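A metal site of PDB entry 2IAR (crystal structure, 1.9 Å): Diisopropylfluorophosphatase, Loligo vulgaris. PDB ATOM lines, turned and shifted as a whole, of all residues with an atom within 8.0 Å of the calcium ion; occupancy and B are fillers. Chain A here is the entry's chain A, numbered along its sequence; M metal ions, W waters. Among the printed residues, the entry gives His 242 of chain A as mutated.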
ATOM      1  N   GLY A  17       9.530  31.731  15.226  1.00  0.00           N
ATOM      2  CA  GLY A  17       9.407  31.225  16.567  1.00  0.00           C
ATOM      3  C   GLY A  17      10.606  31.551  17.443  1.00  0.00           C
ATOM      4  O   GLY A  17      10.822  30.866  18.446  1.00  0.00           O
ATOM      5  N   ALA A  18      11.361  32.592  17.073  1.00  0.00           N
ATOM      6  CA  ALA A  18      12.545  33.070  17.794  1.00  0.00           C
ATOM      7  C   ALA A  18      12.500  32.693  19.268  1.00  0.00           C
ATOM      8  O   ALA A  18      11.693  33.233  20.030  1.00  0.00           O
ATOM      9  CB  ALA A  18      12.683  34.578  17.638  1.00  0.00           C
ATOM     10  N   GLU A  19      13.393  31.794  19.663  1.00  0.00           N
ATOM     11  CA  GLU A  19      13.421  31.283  21.022  1.00  0.00           C
ATOM     12  C   GLU A  19      14.802  30.997  21.602  1.00  0.00           C
ATOM     13  O   GLU A  19      15.829  31.169  20.939  1.00  0.00           O
ATOM     14  CB  GLU A  19      12.624  29.963  21.063  1.00  0.00           C
ATOM     15  CG  GLU A  19      11.199  30.092  21.545  1.00  0.00           C
ATOM     16  CD  GLU A  19      11.087  30.006  23.047  1.00  0.00           C
ATOM     17  OE1 GLU A  19      12.054  30.347  23.766  1.00  0.00           O
ATOM     18  OE2 GLU A  19      10.028  29.563  23.515  1.00  0.00           O
ATOM     19  N   GLY A  20      14.772  30.509  22.838  1.00  0.00           N
ATOM     20  CA  GLY A  20      15.949  30.116  23.592  1.00  0.00           C
ATOM     21  C   GLY A  20      17.240  30.884  23.485  1.00  0.00           C
ATOM     22  O   GLY A  20      18.277  30.257  23.249  1.00  0.00           O
ATOM     23  N   ALA A  72      13.454  24.684  21.040  1.00  0.00           N
ATOM     24  CA  ALA A  72      12.826  25.843  21.668  1.00  0.00           C
ATOM     25  C   ALA A  72      13.493  26.493  22.892  1.00  0.00           C
ATOM     26  O   ALA A  72      13.203  27.643  23.200  1.00  0.00           O
ATOM     27  CB  ALA A  72      11.364  25.503  22.008  1.00  0.00           C
ATOM     28  N   GLY A  73      14.337  25.769  23.612  1.00  0.00           N
ATOM     29  CA  GLY A  73      14.991  26.346  24.778  1.00  0.00           C
ATOM     30  C   GLY A  73      16.434  25.909  24.916  1.00  0.00           C
ATOM     31  O   GLY A  73      16.783  24.795  24.513  1.00  0.00           O
ATOM     32  N   MET A  88      10.939  20.300  20.951  1.00  0.00           N
ATOM     33  CA  MET A  88       9.543  19.857  21.004  1.00  0.00           C
ATOM     34  C   MET A  88       9.236  18.540  20.285  1.00  0.00           C
ATOM     35  O   MET A  88       8.176  17.943  20.491  1.00  0.00           O
ATOM     36  CB  MET A  88       8.597  20.959  20.497  1.00  0.00           C
ATOM     37  CG  MET A  88       8.514  22.205  21.396  1.00  0.00           C
ATOM     38  SD  MET A  88       7.647  21.953  22.985  1.00  0.00           S
ATOM     39  CE  MET A  88       5.912  22.174  22.473  1.00  0.00           C
ATOM     40  N   CYS A 117      10.334  18.588  24.607  1.00  0.00           N
ATOM     41  CA  CYS A 117      10.623  19.618  25.600  1.00  0.00           C
ATOM     42  C   CYS A 117      10.600  21.042  25.055  1.00  0.00           C
ATOM     43  O   CYS A 117      10.717  21.253  23.845  1.00  0.00           O
ATOM     44  CB  CYS A 117      11.971  19.314  26.257  1.00  0.00           C
ATOM     45  SG  CYS A 117      12.015  17.717  27.116  1.00  0.00           S
ATOM     46  N   ASN A 118      10.486  22.016  25.951  1.00  0.00           N
ATOM     47  CA  ASN A 118      10.443  23.416  25.531  1.00  0.00           C
ATOM     48  C   ASN A 118      11.536  24.323  26.089  1.00  0.00           C
ATOM     49  O   ASN A 118      12.094  25.152  25.369  1.00  0.00           O
ATOM     50  CB  ASN A 118       9.077  24.027  25.815  1.00  0.00           C
ATOM     51  CG  ASN A 118       8.881  25.349  25.126  1.00  0.00           C
ATOM     52  OD1 ASN A 118       9.328  26.376  25.607  1.00  0.00           O
ATOM     53  ND2 ASN A 118       8.239  25.314  23.965  1.00  0.00           N
ATOM     54  N   ASP A 119      11.813  24.206  27.389  1.00  0.00           N
ATOM     55  CA  ASP A 119      12.851  25.005  28.010  1.00  0.00           C
ATOM     56  C   ASP A 119      13.498  24.228  29.149  1.00  0.00           C
ATOM     57  O   ASP A 119      12.929  23.247  29.636  1.00  0.00           O
ATOM     58  CB  ASP A 119      12.290  26.339  28.520  1.00  0.00           C
ATOM     59  CG  ASP A 119      13.324  27.467  28.518  1.00  0.00           C
ATOM     60  OD1 ASP A 119      14.524  27.207  28.334  1.00  0.00           O
ATOM     61  OD2 ASP A 119      12.922  28.627  28.675  1.00  0.00           O
ATOM     62  N   CYS A 120      14.676  24.680  29.573  1.00  0.00           N
ATOM     63  CA  CYS A 120      15.418  24.011  30.630  1.00  0.00           C
ATOM     64  C   CYS A 120      16.223  24.996  31.470  1.00  0.00           C
ATOM     65  O   CYS A 120      16.545  26.103  31.014  1.00  0.00           O
ATOM     66  CB  CYS A 120      16.349  22.943  30.046  1.00  0.00           C
ATOM     67  SG  CYS A 120      17.453  23.516  28.745  1.00  0.00           S
ATOM     68  N   THR A 131      11.206  21.430  30.988  1.00  0.00           N
ATOM     69  CA  THR A 131       9.742  21.446  30.846  1.00  0.00           C
ATOM     70  C   THR A 131       9.383  20.700  29.561  1.00  0.00           C
ATOM     71  O   THR A 131       9.991  20.923  28.518  1.00  0.00           O
ATOM     72  CB  THR A 131       9.148  22.879  30.756  1.00  0.00           C
ATOM     73  OG1 THR A 131       9.771  23.601  29.684  1.00  0.00           O
ATOM     74  CG2 THR A 131       9.332  23.612  32.070  1.00  0.00           C
ATOM     75  N   PRO A 133       6.158  20.302  27.460  1.00  0.00           N
ATOM     76  CA  PRO A 133       4.779  20.618  27.070  1.00  0.00           C
ATOM     77  C   PRO A 133       4.177  19.774  25.941  1.00  0.00           C
ATOM     78  O   PRO A 133       2.960  19.667  25.818  1.00  0.00           O
ATOM     79  CB  PRO A 133       4.869  22.093  26.701  1.00  0.00           C
ATOM     80  CG  PRO A 133       6.249  22.209  26.126  1.00  0.00           C
ATOM     81  CD  PRO A 133       7.064  21.419  27.117  1.00  0.00           C
ATOM     82  N   PHE A 171       0.711  22.890  29.444  1.00  0.00           N
ATOM     83  CA  PHE A 171       1.794  23.542  28.734  1.00  0.00           C
ATOM     84  C   PHE A 171       2.854  24.165  29.619  1.00  0.00           C
ATOM     85  O   PHE A 171       2.913  25.396  29.766  1.00  0.00           O
ATOM     86  CB  PHE A 171       1.283  24.548  27.694  1.00  0.00           C
ATOM     87  CG  PHE A 171       2.241  24.764  26.544  1.00  0.00           C
ATOM     88  CD1 PHE A 171       3.273  25.705  26.623  1.00  0.00           C
ATOM     89  CD2 PHE A 171       2.132  24.000  25.379  1.00  0.00           C
ATOM     90  CE1 PHE A 171       4.173  25.874  25.569  1.00  0.00           C
ATOM     91  CE2 PHE A 171       3.018  24.169  24.326  1.00  0.00           C
ATOM     92  CZ  PHE A 171       4.046  25.112  24.427  1.00  0.00           C
ATOM     93  N   PRO A 172       3.686  23.328  30.282  1.00  0.00           N
ATOM     94  CA  PRO A 172       4.751  23.869  31.135  1.00  0.00           C
ATOM     95  C   PRO A 172       5.708  24.545  30.161  1.00  0.00           C
ATOM     96  O   PRO A 172       5.984  24.006  29.086  1.00  0.00           O
ATOM     97  CB  PRO A 172       5.338  22.605  31.774  1.00  0.00           C
ATOM     98  CG  PRO A 172       5.063  21.525  30.767  1.00  0.00           C
ATOM     99  CD  PRO A 172       3.662  21.857  30.322  1.00  0.00           C
ATOM    100  N   ASN A 173       6.168  25.745  30.496  1.00  0.00           N
ATOM    101  CA  ASN A 173       7.018  26.492  29.588  1.00  0.00           C
ATOM    102  C   ASN A 173       8.373  26.906  30.176  1.00  0.00           C
ATOM    103  O   ASN A 173       9.306  26.101  30.220  1.00  0.00           O
ATOM    104  CB  ASN A 173       6.229  27.719  29.097  1.00  0.00           C
ATOM    105  CG  ASN A 173       6.604  28.138  27.702  1.00  0.00           C
ATOM    106  OD1 ASN A 173       7.763  28.078  27.327  1.00  0.00           O
ATOM    107  ND2 ASN A 173       5.629  28.564  26.914  1.00  0.00           N
ATOM    108  N   GLY A 174       8.485  28.162  30.580  1.00  0.00           N
ATOM    109  CA  GLY A 174       9.716  28.653  31.158  1.00  0.00           C
ATOM    110  C   GLY A 174       9.993  27.976  32.488  1.00  0.00           C
ATOM    111  O   GLY A 174       9.075  27.497  33.169  1.00  0.00           O
ATOM    112  N   ILE A 175      11.265  27.917  32.848  1.00  0.00           N
ATOM    113  CA  ILE A 175      11.653  27.269  34.099  1.00  0.00           C
ATOM    114  C   ILE A 175      12.912  27.929  34.643  1.00  0.00           C
ATOM    115  O   ILE A 175      13.742  28.432  33.879  1.00  0.00           O
ATOM    116  CB  ILE A 175      11.844  25.729  33.852  1.00  0.00           C
ATOM    117  CG1 ILE A 175      12.127  24.981  35.163  1.00  0.00           C
ATOM    118  CG2 ILE A 175      12.900  25.481  32.794  1.00  0.00           C
ATOM    119  CD1 ILE A 175      11.996  23.489  35.032  1.00  0.00           C
ATOM    120  N   THR A 193       1.888  28.242  30.894  1.00  0.00           N
ATOM    121  CA  THR A 193       1.386  29.265  29.987  1.00  0.00           C
ATOM    122  C   THR A 193      -0.092  29.678  29.975  1.00  0.00           C
ATOM    123  O   THR A 193      -0.439  30.700  30.547  1.00  0.00           O
ATOM    124  CB  THR A 193       1.902  29.064  28.543  1.00  0.00           C
ATOM    125  OG1 THR A 193       3.326  28.891  28.570  1.00  0.00           O
ATOM    126  CG2 THR A 193       1.574  30.284  27.690  1.00  0.00           C
ATOM    127  N   ALA A 226       2.730  33.231  30.684  1.00  0.00           N
ATOM    128  CA  ALA A 226       4.150  33.131  30.972  1.00  0.00           C
ATOM    129  C   ALA A 226       4.882  32.199  30.012  1.00  0.00           C
ATOM    130  O   ALA A 226       4.452  31.063  29.762  1.00  0.00           O
ATOM    131  CB  ALA A 226       4.379  32.679  32.409  1.00  0.00           C
ATOM    132  N   ASP A 227       5.964  32.698  29.445  1.00  0.00           N
ATOM    133  CA  ASP A 227       6.778  31.920  28.531  1.00  0.00           C
ATOM    134  C   ASP A 227       8.156  31.727  29.157  1.00  0.00           C
ATOM    135  O   ASP A 227       8.289  30.947  30.111  1.00  0.00           O
ATOM    136  CB  ASP A 227       6.851  32.613  27.158  1.00  0.00           C
ATOM    137  CG  ASP A 227       7.381  31.710  26.064  1.00  0.00           C
ATOM    138  OD1 ASP A 227       8.172  30.804  26.380  1.00  0.00           O
ATOM    139  OD2 ASP A 227       7.010  31.890  24.880  1.00  0.00           O
ATOM    140  N   GLY A 228       9.174  32.459  28.686  1.00  0.00           N
ATOM    141  CA  GLY A 228      10.520  32.331  29.234  1.00  0.00           C
ATOM    142  C   GLY A 228      10.779  33.104  30.516  1.00  0.00           C
ATOM    143  O   GLY A 228      10.103  34.093  30.795  1.00  0.00           O
ATOM    144  N   MET A 229      11.772  32.667  31.280  1.00  0.00           N
ATOM    145  CA  MET A 229      12.102  33.321  32.546  1.00  0.00           C
ATOM    146  C   MET A 229      13.571  33.207  32.935  1.00  0.00           C
ATOM    147  O   MET A 229      14.295  32.349  32.436  1.00  0.00           O
ATOM    148  CB  MET A 229      11.235  32.767  33.688  1.00  0.00           C
ATOM    149  CG  MET A 229      11.509  31.308  34.012  1.00  0.00           C
ATOM    150  SD  MET A 229      10.561  30.674  35.411  1.00  0.00           S
ATOM    151  CE  MET A 229       8.916  30.893  34.817  1.00  0.00           C
ATOM    152  N   HIS A 242       3.932  36.347  27.172  1.00  0.00           N
ATOM    153  CA  HIS A 242       3.560  36.195  25.756  1.00  0.00           C
ATOM    154  C   HIS A 242       2.120  36.615  25.468  1.00  0.00           C
ATOM    155  O   HIS A 242       1.180  36.005  25.959  1.00  0.00           O
ATOM    156  CB  HIS A 242       3.786  34.737  25.343  1.00  0.00           C
ATOM    157  CG  HIS A 242       3.899  34.525  23.864  1.00  0.00           C
ATOM    158  ND1 HIS A 242       2.822  34.604  23.007  1.00  0.00           N
ATOM    159  CD2 HIS A 242       4.958  34.182  23.103  1.00  0.00           C
ATOM    160  CE1 HIS A 242       3.211  34.311  21.784  1.00  0.00           C
ATOM    161  NE2 HIS A 242       4.502  34.044  21.811  1.00  0.00           N
ATOM    162  N   SER A 269       8.780  36.332  23.901  1.00  0.00           N
ATOM    163  CA  SER A 269       8.893  34.904  24.136  1.00  0.00           C
ATOM    164  C   SER A 269       9.881  34.463  25.201  1.00  0.00           C
ATOM    165  O   SER A 269       9.501  33.832  26.181  1.00  0.00           O
ATOM    166  CB  SER A 269       9.222  34.185  22.829  1.00  0.00           C
ATOM    167  OG  SER A 269       9.383  32.808  23.062  1.00  0.00           O
ATOM    168  N   ASN A 270      11.155  34.775  25.007  1.00  0.00           N
ATOM    169  CA  ASN A 270      12.179  34.359  25.959  1.00  0.00           C
ATOM    170  C   ASN A 270      13.201  35.466  26.152  1.00  0.00           C
ATOM    171  O   ASN A 270      13.225  36.440  25.404  1.00  0.00           O
ATOM    172  CB  ASN A 270      12.874  33.078  25.451  1.00  0.00           C
ATOM    173  CG  ASN A 270      13.146  32.061  26.571  1.00  0.00           C
ATOM    174  OD1 ASN A 270      13.049  30.845  26.356  1.00  0.00           O
ATOM    175  ND2 ASN A 270      13.503  32.550  27.749  1.00  0.00           N
ATOM    176  N   THR A 283      13.551  37.608  22.804  1.00  0.00           N
ATOM    177  CA  THR A 283      13.017  37.071  21.578  1.00  0.00           C
ATOM    178  C   THR A 283      11.502  37.286  21.632  1.00  0.00           C
ATOM    179  O   THR A 283      10.911  37.247  22.720  1.00  0.00           O
ATOM    180  CB  THR A 283      13.354  35.569  21.419  1.00  0.00           C
ATOM    181  OG1 THR A 283      12.790  34.829  22.512  1.00  0.00           O
ATOM    182  CG2 THR A 283      14.848  35.374  21.374  1.00  0.00           C
ATOM    183  N   HIS A 285       7.614  36.845  19.230  1.00  0.00           N
ATOM    184  CA  HIS A 285       6.929  36.229  18.091  1.00  0.00           C
ATOM    185  C   HIS A 285       6.002  37.084  17.239  1.00  0.00           C
ATOM    186  O   HIS A 285       5.326  36.551  16.359  1.00  0.00           O
ATOM    187  CB  HIS A 285       6.198  34.973  18.563  1.00  0.00           C
ATOM    188  CG  HIS A 285       7.103  33.967  19.213  1.00  0.00           C
ATOM    189  ND1 HIS A 285       6.643  32.987  20.064  1.00  0.00           N
ATOM    190  CD2 HIS A 285       8.444  33.796  19.136  1.00  0.00           C
ATOM    191  CE1 HIS A 285       7.656  32.263  20.486  1.00  0.00           C
ATOM    192  NE2 HIS A 285       8.763  32.734  19.939  1.00  0.00           N
HETATM  193 CA    CA M   1       9.355  28.760  25.782  1.00  0.00          CA
HETATM  194  O   HOH W   1       7.269  28.915  24.160  1.00  0.00           O
HETATM  195  O   HOH W   2      11.826  27.998  25.541  1.00  0.00           O
HETATM  196  O   HOH W   3      10.493  29.261  27.976  1.00  0.00           O
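The calcium ion is bound by OD1 of Asn 173 (2.3 Å).
The calcium ion is bound by the side-chain amide oxygen (OD1) of Asn 118, at 2.4 Å.
The calcium ion is bound by OD1 of Asp 227, at 2.4 Å.
The calcium ion is bound by OE2 of Glu 19 (2.5 Å).
Water W3 is bound to the calcium ion.
Water W2 is bound to the calcium ion, at 2.6 Å.
Water W1 is bound to the calcium ion (2.6 Å).
The calcium ion has seven donor atoms within binding distance.
The backbone NH of Asn 118 lies within hydrogen-bond range of the backbone carbonyl oxygen of Thr 131, at 2.8 Å.
The side-chain amide nitrogen of Asn 118 sits at hydrogen-bond distance from the side-chain sulfur of Met 88.
OG1 of Thr 131 lies within hydrogen-bond range of O of Asn 173, at 2.6 Å.
The side-chain carboxylate (OD2) of Asp 227 lies within hydrogen-bond range of the side-chain hydroxyl (OG) of Ser 269 (3.1 Å).
The side-chain amide oxygen of Asn 270 lies close to the side-chain carboxylate of Glu 19 (2.8 Å).
The backbone carbonyl oxygen of Asn 118 sits at hydrogen-bond distance from the backbone NH of Gly 73 (2.9 Å).
O of Asp 227 sits at hydrogen-bond distance from N of Gly 174, at 2.8 Å.
The side-chain hydroxyl of Thr 193 sits at hydrogen-bond distance from the side-chain amide nitrogen of Asn 173, 2.9 Å away.
Water W1 lies within hydrogen-bond range of OD2 of Asp 227 (3.1 Å) and ND2 of Asn 173 (3.2 Å).
Water W3 lies within hydrogen-bond range of the side-chain carboxylate of Asp 119 (2.6 Å), the side-chain amide oxygen of Asn 270 (3.4 Å) and the backbone NH of Gly 174 (3.5 Å).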
